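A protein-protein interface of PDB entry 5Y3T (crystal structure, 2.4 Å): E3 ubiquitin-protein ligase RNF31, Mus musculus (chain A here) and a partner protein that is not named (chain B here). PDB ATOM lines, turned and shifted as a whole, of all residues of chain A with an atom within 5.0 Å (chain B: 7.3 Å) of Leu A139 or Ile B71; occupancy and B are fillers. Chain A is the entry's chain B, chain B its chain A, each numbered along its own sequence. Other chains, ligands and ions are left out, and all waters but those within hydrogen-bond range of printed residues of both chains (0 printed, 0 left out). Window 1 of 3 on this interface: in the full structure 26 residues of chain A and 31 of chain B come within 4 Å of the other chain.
OE1 of Gln A135 lies within hydrogen-bond range of N of Trp B72 (2.9 Å). The backbone carbonyl oxygen (O) of Asp B91 is in hydrogen-bond range of the guanidinium group (NH2) of Arg A136.
The backbone NH (N) of Val B59 sits at hydrogen-bond distance from the backbone carbonyl oxygen (O) of Ile B71 (3.0 Å). The backbone carbonyl oxygen (O) of Val B69 lies within hydrogen-bond range of the backbone NH (N) of Val B61.
Among the printed residues, pairs that only touch across the chains: Gln A135 with Ile B71 (3.4 Å), Gln A135 with Tyr B92 (3.9 Å), Arg A138 with Val B69 (3.9 Å), Leu A139 with Ile B71 (3.8 Å), Leu A139 with Tyr B92 (3.3 Å), Leu A139 with Phe B94 (3.7 Å), Phe A142 with Val B69 (3.6 Å), Phe A142 with Phe B94 (3.7 Å), His A143 with Tyr B92 (3.7 Å) and His A143 with Phe B94 (3.5 Å).
Leu A139 touches just these residues of chain B: Ile B71 (3.8 Å), Tyr B92 (3.3 Å) and Phe B94 (3.7 Å). Printed residues of chain B within 4 Å of Phe A142: Val B69 (3.6 Å) and Phe B94 (3.7 Å). Of the printed residues of chain B, Arg A138 touches Val B69. Of the printed residues of chain B, Arg A136 touches Asp B91. Of the printed residues of chain A, Asp B91 touches Arg A136. Printed residues of chain B within 4 Å of His A143: Tyr B92 (3.7 Å) and Phe B94 (3.5 Å). Ser B60 touches none of the printed residues of chain A. The nearest residue of chain B that does not touch Leu A139 is Val B69 (4.3 Å).
Of the 18 printed residues of chain B, 6 touch a printed residue of chain A. Printed residues of chain B that touch a printed residue of chain A: Val B69, Ile B71, Trp B72, Asp B91, Tyr B92 and Phe B94. Hydrophobic or aromatic side chains of chain B that line the printed part of chain A: Val B69, Ile B71, Trp B72, Tyr B92 and Phe B94. Of the 9 printed residues of chain A, 6 touch a printed residue of chain B. Among the printed residues, 12 pairs touch across the chains. Among the printed residues, no Asp or Glu carboxylate lies within 4 Å of a Lys or Arg side-chain nitrogen of the other chain.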
ATOM      1  N   GLN A 135      24.045   0.798 -28.101  1.00  0.00           N
ATOM      2  CA  GLN A 135      23.497  -0.412 -27.479  1.00  0.00           C
ATOM      3  C   GLN A 135      22.472  -1.134 -28.339  1.00  0.00           C
ATOM      4  O   GLN A 135      21.969  -2.193 -27.939  1.00  0.00           O
ATOM      5  CB  GLN A 135      22.867  -0.072 -26.149  1.00  0.00           C
ATOM      6  CG  GLN A 135      23.884   0.323 -25.098  1.00  0.00           C
ATOM      7  CD  GLN A 135      23.218   0.719 -23.800  1.00  0.00           C
ATOM      8  OE1 GLN A 135      23.553   0.216 -22.735  1.00  0.00           O
ATOM      9  NE2 GLN A 135      22.241   1.574 -23.894  1.00  0.00           N
ATOM     10  N   ARG A 136      22.164  -0.584 -29.504  1.00  0.00           N
ATOM     11  CA  ARG A 136      21.327  -1.289 -30.445  1.00  0.00           C
ATOM     12  C   ARG A 136      21.779  -2.724 -30.646  1.00  0.00           C
ATOM     13  O   ARG A 136      20.971  -3.646 -30.473  1.00  0.00           O
ATOM     14  CB  ARG A 136      21.241  -0.563 -31.779  1.00  0.00           C
ATOM     15  CG  ARG A 136      20.245   0.582 -31.741  1.00  0.00           C
ATOM     16  CD  ARG A 136      19.542   0.864 -33.077  1.00  0.00           C
ATOM     17  NE  ARG A 136      18.342   1.610 -32.753  1.00  0.00           N
ATOM     18  CZ  ARG A 136      18.314   2.900 -32.438  1.00  0.00           C
ATOM     19  NH1 ARG A 136      19.431   3.668 -32.478  1.00  0.00           N
ATOM     20  NH2 ARG A 136      17.156   3.441 -32.081  1.00  0.00           N
ATOM     21  N   GLN A 137      23.051  -2.933 -30.943  1.00  0.00           N
ATOM     22  CA  GLN A 137      23.533  -4.318 -31.174  1.00  0.00           C
ATOM     23  C   GLN A 137      23.306  -5.253 -29.991  1.00  0.00           C
ATOM     24  O   GLN A 137      23.061  -6.435 -30.181  1.00  0.00           O
ATOM     25  CB  GLN A 137      24.992  -4.348 -31.591  1.00  0.00           C
ATOM     26  CG  GLN A 137      25.172  -4.042 -33.076  1.00  0.00           C
ATOM     27  CD  GLN A 137      26.522  -4.491 -33.628  1.00  0.00           C
ATOM     28  OE1 GLN A 137      27.497  -4.662 -32.884  1.00  0.00           O
ATOM     29  NE2 GLN A 137      26.583  -4.680 -34.940  1.00  0.00           N
ATOM     30  N   ARG A 138      23.363  -4.723 -28.773  1.00  0.00           N
ATOM     31  CA  ARG A 138      23.124  -5.536 -27.613  1.00  0.00           C
ATOM     32  C   ARG A 138      21.666  -6.032 -27.577  1.00  0.00           C
ATOM     33  O   ARG A 138      21.448  -7.140 -27.115  1.00  0.00           O
ATOM     34  CB  ARG A 138      23.467  -4.779 -26.328  1.00  0.00           C
ATOM     35  CG  ARG A 138      24.923  -4.837 -26.005  1.00  0.00           C
ATOM     36  CD  ARG A 138      25.361  -3.881 -24.900  1.00  0.00           C
ATOM     37  NE  ARG A 138      26.805  -4.029 -24.756  1.00  0.00           N
ATOM     38  CZ  ARG A 138      27.422  -5.055 -24.147  1.00  0.00           C
ATOM     39  NH1 ARG A 138      26.731  -6.046 -23.542  1.00  0.00           N
ATOM     40  NH2 ARG A 138      28.760  -5.086 -24.122  1.00  0.00           N
ATOM     41  N   LEU A 139      20.687  -5.227 -28.020  1.00  0.00           N
ATOM     42  CA  LEU A 139      19.257  -5.612 -27.888  1.00  0.00           C
ATOM     43  C   LEU A 139      18.691  -6.331 -29.102  1.00  0.00           C
ATOM     44  O   LEU A 139      17.653  -6.970 -29.016  1.00  0.00           O
ATOM     45  CB  LEU A 139      18.383  -4.418 -27.500  1.00  0.00           C
ATOM     46  CG  LEU A 139      18.653  -3.871 -26.091  1.00  0.00           C
ATOM     47  CD1 LEU A 139      17.947  -2.546 -25.838  1.00  0.00           C
ATOM     48  CD2 LEU A 139      18.285  -4.882 -25.012  1.00  0.00           C
ATOM     49  N   GLU A 140      19.389  -6.281 -30.223  1.00  0.00           N
ATOM     50  CA  GLU A 140      18.922  -6.973 -31.422  1.00  0.00           C
ATOM     51  C   GLU A 140      18.590  -8.444 -31.229  1.00  0.00           C
ATOM     52  O   GLU A 140      17.564  -8.879 -31.674  1.00  0.00           O
ATOM     53  CB  GLU A 140      19.917  -6.816 -32.604  1.00  0.00           C
ATOM     54  CG  GLU A 140      19.785  -5.461 -33.278  1.00  0.00           C
ATOM     55  CD  GLU A 140      20.982  -5.053 -34.136  1.00  0.00           C
ATOM     56  OE1 GLU A 140      22.030  -5.724 -34.161  1.00  0.00           O
ATOM     57  OE2 GLU A 140      20.857  -4.011 -34.790  1.00  0.00           O
ATOM     58  N   PRO A 141      19.478  -9.214 -30.608  1.00  0.00           N
ATOM     59  CA  PRO A 141      19.122 -10.623 -30.423  1.00  0.00           C
ATOM     60  C   PRO A 141      17.911 -10.829 -29.496  1.00  0.00           C
ATOM     61  O   PRO A 141      17.167 -11.792 -29.693  1.00  0.00           O
ATOM     62  CB  PRO A 141      20.388 -11.259 -29.832  1.00  0.00           C
ATOM     63  CG  PRO A 141      21.469 -10.234 -29.976  1.00  0.00           C
ATOM     64  CD  PRO A 141      20.789  -8.891 -30.017  1.00  0.00           C
ATOM     65  N   PHE A 142      17.659  -9.910 -28.571  1.00  0.00           N
ATOM     66  CA  PHE A 142      16.435  -9.969 -27.758  1.00  0.00           C
ATOM     67  C   PHE A 142      15.249  -9.696 -28.637  1.00  0.00           C
ATOM     68  O   PHE A 142      14.222 -10.377 -28.561  1.00  0.00           O
ATOM     69  CB  PHE A 142      16.511  -9.006 -26.582  1.00  0.00           C
ATOM     70  CG  PHE A 142      17.492  -9.456 -25.519  1.00  0.00           C
ATOM     71  CD1 PHE A 142      18.849  -9.249 -25.670  1.00  0.00           C
ATOM     72  CD2 PHE A 142      17.033 -10.122 -24.356  1.00  0.00           C
ATOM     73  CE1 PHE A 142      19.755  -9.671 -24.693  1.00  0.00           C
ATOM     74  CE2 PHE A 142      17.944 -10.554 -23.390  1.00  0.00           C
ATOM     75  CZ  PHE A 142      19.303 -10.314 -23.553  1.00  0.00           C
ATOM     76  N   HIS A 143      15.403  -8.754 -29.559  1.00  0.00           N
ATOM     77  CA  HIS A 143      14.317  -8.542 -30.517  1.00  0.00           C
ATOM     78  C   HIS A 143      14.085  -9.756 -31.402  1.00  0.00           C
ATOM     79  O   HIS A 143      12.925 -10.129 -31.656  1.00  0.00           O
ATOM     80  CB  HIS A 143      14.509  -7.290 -31.362  1.00  0.00           C
ATOM     81  CG  HIS A 143      13.273  -6.874 -32.081  1.00  0.00           C
ATOM     82  ND1 HIS A 143      12.964  -7.326 -33.348  1.00  0.00           N
ATOM     83  CD2 HIS A 143      12.257  -6.066 -31.708  1.00  0.00           C
ATOM     84  CE1 HIS A 143      11.807  -6.807 -33.720  1.00  0.00           C
ATOM     85  NE2 HIS A 143      11.360  -6.041 -32.742  1.00  0.00           N
ATOM     86  N   LEU B  57      20.004   5.035 -15.910  1.00  0.00           N
ATOM     87  CA  LEU B  57      19.419   3.909 -15.172  1.00  0.00           C
ATOM     88  C   LEU B  57      20.073   2.600 -15.602  1.00  0.00           C
ATOM     89  O   LEU B  57      20.079   2.266 -16.768  1.00  0.00           O
ATOM     90  CB  LEU B  57      17.915   3.821 -15.434  1.00  0.00           C
ATOM     91  CG  LEU B  57      17.194   2.516 -15.037  1.00  0.00           C
ATOM     92  CD1 LEU B  57      17.149   2.413 -13.530  1.00  0.00           C
ATOM     93  CD2 LEU B  57      15.794   2.428 -15.624  1.00  0.00           C
ATOM     94  N   CYS B  58      20.577   1.842 -14.650  1.00  0.00           N
ATOM     95  CA  CYS B  58      21.147   0.546 -14.931  1.00  0.00           C
ATOM     96  C   CYS B  58      20.059  -0.528 -14.930  1.00  0.00           C
ATOM     97  O   CYS B  58      19.600  -0.981 -13.881  1.00  0.00           O
ATOM     98  CB  CYS B  58      22.278   0.213 -13.951  1.00  0.00           C
ATOM     99  SG  CYS B  58      23.084  -1.347 -14.366  1.00  0.00           S
ATOM    100  N   VAL B  59      19.665  -0.941 -16.134  1.00  0.00           N
ATOM    101  CA  VAL B  59      18.597  -1.890 -16.329  1.00  0.00           C
ATOM    102  C   VAL B  59      19.183  -3.264 -16.537  1.00  0.00           C
ATOM    103  O   VAL B  59      19.916  -3.453 -17.492  1.00  0.00           O
ATOM    104  CB  VAL B  59      17.770  -1.548 -17.592  1.00  0.00           C
ATOM    105  CG1 VAL B  59      16.664  -2.562 -17.813  1.00  0.00           C
ATOM    106  CG2 VAL B  59      17.204  -0.139 -17.514  1.00  0.00           C
ATOM    107  N   SER B  60      18.826  -4.214 -15.667  1.00  0.00           N
ATOM    108  CA  SER B  60      19.009  -5.628 -15.922  1.00  0.00           C
ATOM    109  C   SER B  60      17.845  -6.131 -16.784  1.00  0.00           C
ATOM    110  O   SER B  60      16.694  -6.004 -16.402  1.00  0.00           O
ATOM    111  CB  SER B  60      18.989  -6.430 -14.611  1.00  0.00           C
ATOM    112  OG  SER B  60      19.739  -5.775 -13.644  1.00  0.00           O
ATOM    113  N   VAL B  61      18.159  -6.764 -17.903  1.00  0.00           N
ATOM    114  CA  VAL B  61      17.180  -7.253 -18.826  1.00  0.00           C
ATOM    115  C   VAL B  61      17.286  -8.763 -18.840  1.00  0.00           C
ATOM    116  O   VAL B  61      18.362  -9.290 -18.981  1.00  0.00           O
ATOM    117  CB  VAL B  61      17.443  -6.748 -20.256  1.00  0.00           C
ATOM    118  CG1 VAL B  61      16.380  -7.265 -21.229  1.00  0.00           C
ATOM    119  CG2 VAL B  61      17.511  -5.251 -20.282  1.00  0.00           C
ATOM    120  N   VAL B  69      21.120  -9.434 -20.061  1.00  0.00           N
ATOM    121  CA  VAL B  69      22.065  -8.440 -20.507  1.00  0.00           C
ATOM    122  C   VAL B  69      21.805  -7.181 -19.696  1.00  0.00           C
ATOM    123  O   VAL B  69      20.670  -6.962 -19.313  1.00  0.00           O
ATOM    124  CB  VAL B  69      21.933  -8.163 -22.039  1.00  0.00           C
ATOM    125  CG1 VAL B  69      20.820  -7.159 -22.353  1.00  0.00           C
ATOM    126  CG2 VAL B  69      23.267  -7.685 -22.609  1.00  0.00           C
ATOM    127  N   THR B  70      22.840  -6.371 -19.444  1.00  0.00           N
ATOM    128  CA  THR B  70      22.696  -5.050 -18.780  1.00  0.00           C
ATOM    129  C   THR B  70      22.818  -3.937 -19.844  1.00  0.00           C
ATOM    130  O   THR B  70      23.760  -3.957 -20.644  1.00  0.00           O
ATOM    131  CB  THR B  70      23.796  -4.832 -17.715  1.00  0.00           C
ATOM    132  OG1 THR B  70      23.741  -5.861 -16.713  1.00  0.00           O
ATOM    133  CG2 THR B  70      23.618  -3.530 -17.045  1.00  0.00           C
ATOM    134  N   ILE B  71      21.831  -3.033 -19.879  1.00  0.00           N
ATOM    135  CA  ILE B  71      21.840  -1.834 -20.705  1.00  0.00           C
ATOM    136  C   ILE B  71      21.589  -0.628 -19.838  1.00  0.00           C
ATOM    137  O   ILE B  71      21.076  -0.741 -18.736  1.00  0.00           O
ATOM    138  CB  ILE B  71      20.739  -1.814 -21.787  1.00  0.00           C
ATOM    139  CG1 ILE B  71      19.404  -1.399 -21.164  1.00  0.00           C
ATOM    140  CG2 ILE B  71      20.665  -3.143 -22.541  1.00  0.00           C
ATOM    141  CD1 ILE B  71      18.228  -1.528 -22.080  1.00  0.00           C
ATOM    142  N   TRP B  72      21.894   0.537 -20.389  1.00  0.00           N
ATOM    143  CA  TRP B  72      21.789   1.804 -19.709  1.00  0.00           C
ATOM    144  C   TRP B  72      20.801   2.704 -20.410  1.00  0.00           C
ATOM    145  O   TRP B  72      21.009   3.048 -21.553  1.00  0.00           O
ATOM    146  CB  TRP B  72      23.137   2.468 -19.745  1.00  0.00           C
ATOM    147  CG  TRP B  72      24.149   1.844 -18.855  1.00  0.00           C
ATOM    148  CD1 TRP B  72      25.099   0.937 -19.196  1.00  0.00           C
ATOM    149  CD2 TRP B  72      24.351   2.145 -17.464  1.00  0.00           C
ATOM    150  NE1 TRP B  72      25.896   0.647 -18.094  1.00  0.00           N
ATOM    151  CE2 TRP B  72      25.449   1.370 -17.022  1.00  0.00           C
ATOM    152  CE3 TRP B  72      23.714   3.008 -16.553  1.00  0.00           C
ATOM    153  CZ2 TRP B  72      25.908   1.412 -15.721  1.00  0.00           C
ATOM    154  CZ3 TRP B  72      24.176   3.066 -15.269  1.00  0.00           C
ATOM    155  CH2 TRP B  72      25.278   2.274 -14.855  1.00  0.00           C
ATOM    156  N   LEU B  73      19.729   3.096 -19.725  1.00  0.00           N
ATOM    157  CA  LEU B  73      18.786   4.077 -20.255  1.00  0.00           C
ATOM    158  C   LEU B  73      18.957   5.459 -19.627  1.00  0.00           C
ATOM    159  O   LEU B  73      19.476   5.623 -18.529  1.00  0.00           O
ATOM    160  CB  LEU B  73      17.341   3.599 -20.043  1.00  0.00           C
ATOM    161  CG  LEU B  73      17.030   2.241 -20.696  1.00  0.00           C
ATOM    162  CD1 LEU B  73      15.591   1.838 -20.387  1.00  0.00           C
ATOM    163  CD2 LEU B  73      17.298   2.252 -22.206  1.00  0.00           C
ATOM    164  N   VAL B  88      11.359   2.756 -24.583  1.00  0.00           N
ATOM    165  CA  VAL B  88      11.972   1.485 -24.984  1.00  0.00           C
ATOM    166  C   VAL B  88      11.329   0.860 -26.244  1.00  0.00           C
ATOM    167  O   VAL B  88      12.008   0.175 -27.018  1.00  0.00           O
ATOM    168  CB  VAL B  88      12.005   0.510 -23.795  1.00  0.00           C
ATOM    169  CG1 VAL B  88      12.299  -0.922 -24.199  1.00  0.00           C
ATOM    170  CG2 VAL B  88      13.060   0.993 -22.822  1.00  0.00           C
ATOM    171  N   ASP B  91      12.716   3.250 -29.154  1.00  0.00           N
ATOM    172  CA  ASP B  91      14.128   3.109 -29.387  1.00  0.00           C
ATOM    173  C   ASP B  91      14.490   1.752 -29.962  1.00  0.00           C
ATOM    174  O   ASP B  91      15.267   1.683 -30.909  1.00  0.00           O
ATOM    175  CB  ASP B  91      14.913   3.398 -28.102  1.00  0.00           C
ATOM    176  CG  ASP B  91      14.926   4.869 -27.747  1.00  0.00           C
ATOM    177  OD1 ASP B  91      14.697   5.707 -28.669  1.00  0.00           O
ATOM    178  OD2 ASP B  91      15.155   5.198 -26.542  1.00  0.00           O
ATOM    179  N   TYR B  92      13.941   0.684 -29.385  1.00  0.00           N
ATOM    180  CA  TYR B  92      14.348  -0.699 -29.690  1.00  0.00           C
ATOM    181  C   TYR B  92      13.238  -1.642 -30.113  1.00  0.00           C
ATOM    182  O   TYR B  92      13.515  -2.837 -30.365  1.00  0.00           O
ATOM    183  CB  TYR B  92      14.983  -1.288 -28.451  1.00  0.00           C
ATOM    184  CG  TYR B  92      16.074  -0.442 -27.857  1.00  0.00           C
ATOM    185  CD1 TYR B  92      17.206  -0.175 -28.591  1.00  0.00           C
ATOM    186  CD2 TYR B  92      15.998   0.051 -26.564  1.00  0.00           C
ATOM    187  CE1 TYR B  92      18.245   0.547 -28.064  1.00  0.00           C
ATOM    188  CE2 TYR B  92      17.047   0.785 -26.029  1.00  0.00           C
ATOM    189  CZ  TYR B  92      18.152   1.046 -26.823  1.00  0.00           C
ATOM    190  OH  TYR B  92      19.215   1.776 -26.407  1.00  0.00           O
ATOM    191  N   PHE B  94      10.548  -3.114 -28.567  1.00  0.00           N
ATOM    192  CA  PHE B  94       9.816  -4.046 -27.635  1.00  0.00           C
ATOM    193  C   PHE B  94       8.483  -3.421 -27.261  1.00  0.00           C
ATOM    194  O   PHE B  94       8.452  -2.297 -26.691  1.00  0.00           O
ATOM    195  CB  PHE B  94      10.641  -4.374 -26.373  1.00  0.00           C
ATOM    196  CG  PHE B  94      11.952  -4.947 -26.697  1.00  0.00           C
ATOM    197  CD1 PHE B  94      12.032  -6.240 -27.155  1.00  0.00           C
ATOM    198  CD2 PHE B  94      13.082  -4.153 -26.703  1.00  0.00           C
ATOM    199  CE1 PHE B  94      13.234  -6.762 -27.581  1.00  0.00           C
ATOM    200  CE2 PHE B  94      14.303  -4.662 -27.106  1.00  0.00           C
ATOM    201  CZ  PHE B  94      14.379  -5.963 -27.562  1.00  0.00           C
ATOM    202  N   TRP B 101       8.159  -4.292 -15.922  1.00  0.00           N
ATOM    203  CA  TRP B 101       9.155  -3.622 -15.117  1.00  0.00           C
ATOM    204  C   TRP B 101       9.002  -4.026 -13.631  1.00  0.00           C
ATOM    205  O   TRP B 101       7.878  -4.130 -13.092  1.00  0.00           O
ATOM    206  CB  TRP B 101       9.071  -2.107 -15.312  1.00  0.00           C
ATOM    207  CG  TRP B 101       9.613  -1.646 -16.643  1.00  0.00           C
ATOM    208  CD1 TRP B 101       8.897  -1.472 -17.792  1.00  0.00           C
ATOM    209  CD2 TRP B 101      10.968  -1.275 -16.963  1.00  0.00           C
ATOM    210  NE1 TRP B 101       9.706  -1.009 -18.795  1.00  0.00           N
ATOM    211  CE2 TRP B 101      10.980  -0.872 -18.320  1.00  0.00           C
ATOM    212  CE3 TRP B 101      12.158  -1.213 -16.234  1.00  0.00           C
ATOM    213  CZ2 TRP B 101      12.156  -0.460 -18.982  1.00  0.00           C
ATOM    214  CZ3 TRP B 101      13.324  -0.796 -16.877  1.00  0.00           C
ATOM    215  CH2 TRP B 101      13.313  -0.423 -18.243  1.00  0.00           C
ATOM    216  N   ALA B 126      17.076  -1.110 -12.222  1.00  0.00           N
ATOM    217  CA  ALA B 126      15.777  -1.720 -12.450  1.00  0.00           C
ATOM    218  C   ALA B 126      15.950  -2.952 -13.283  1.00  0.00           C
ATOM    219  O   ALA B 126      16.986  -3.165 -13.878  1.00  0.00           O
ATOM    220  CB  ALA B 126      14.826  -0.760 -13.126  1.00  0.00           C
ATOM    221  N   LEU B 128      14.068  -5.235 -16.245  1.00  0.00           N
ATOM    222  CA  LEU B 128      13.099  -5.322 -17.329  1.00  0.00           C
ATOM    223  C   LEU B 128      13.014  -6.760 -17.676  1.00  0.00           C
ATOM    224  O   LEU B 128      14.035  -7.345 -18.008  1.00  0.00           O
ATOM    225  CB  LEU B 128      13.590  -4.577 -18.564  1.00  0.00           C
ATOM    226  CG  LEU B 128      12.841  -4.742 -19.907  1.00  0.00           C
ATOM    227  CD1 LEU B 128      11.355  -4.538 -19.719  1.00  0.00           C
ATOM    228  CD2 LEU B 128      13.394  -3.747 -20.945  1.00  0.00           C
ATOM    229  N   LEU B 130      11.313  -9.327 -20.393  1.00  0.00           N
ATOM    230  CA  LEU B 130      10.727  -9.219 -21.764  1.00  0.00           C
ATOM    231  C   LEU B 130      10.001 -10.465 -22.042  1.00  0.00           C
ATOM    232  O   LEU B 130      10.581 -11.550 -21.993  1.00  0.00           O
ATOM    233  CB  LEU B 130      11.781  -9.007 -22.885  1.00  0.00           C
ATOM    234  CG  LEU B 130      12.409  -7.618 -22.841  1.00  0.00           C
ATOM    235  CD1 LEU B 130      13.646  -7.577 -23.711  1.00  0.00           C
ATOM    236  CD2 LEU B 130      11.433  -6.517 -23.234  1.00  0.00           C
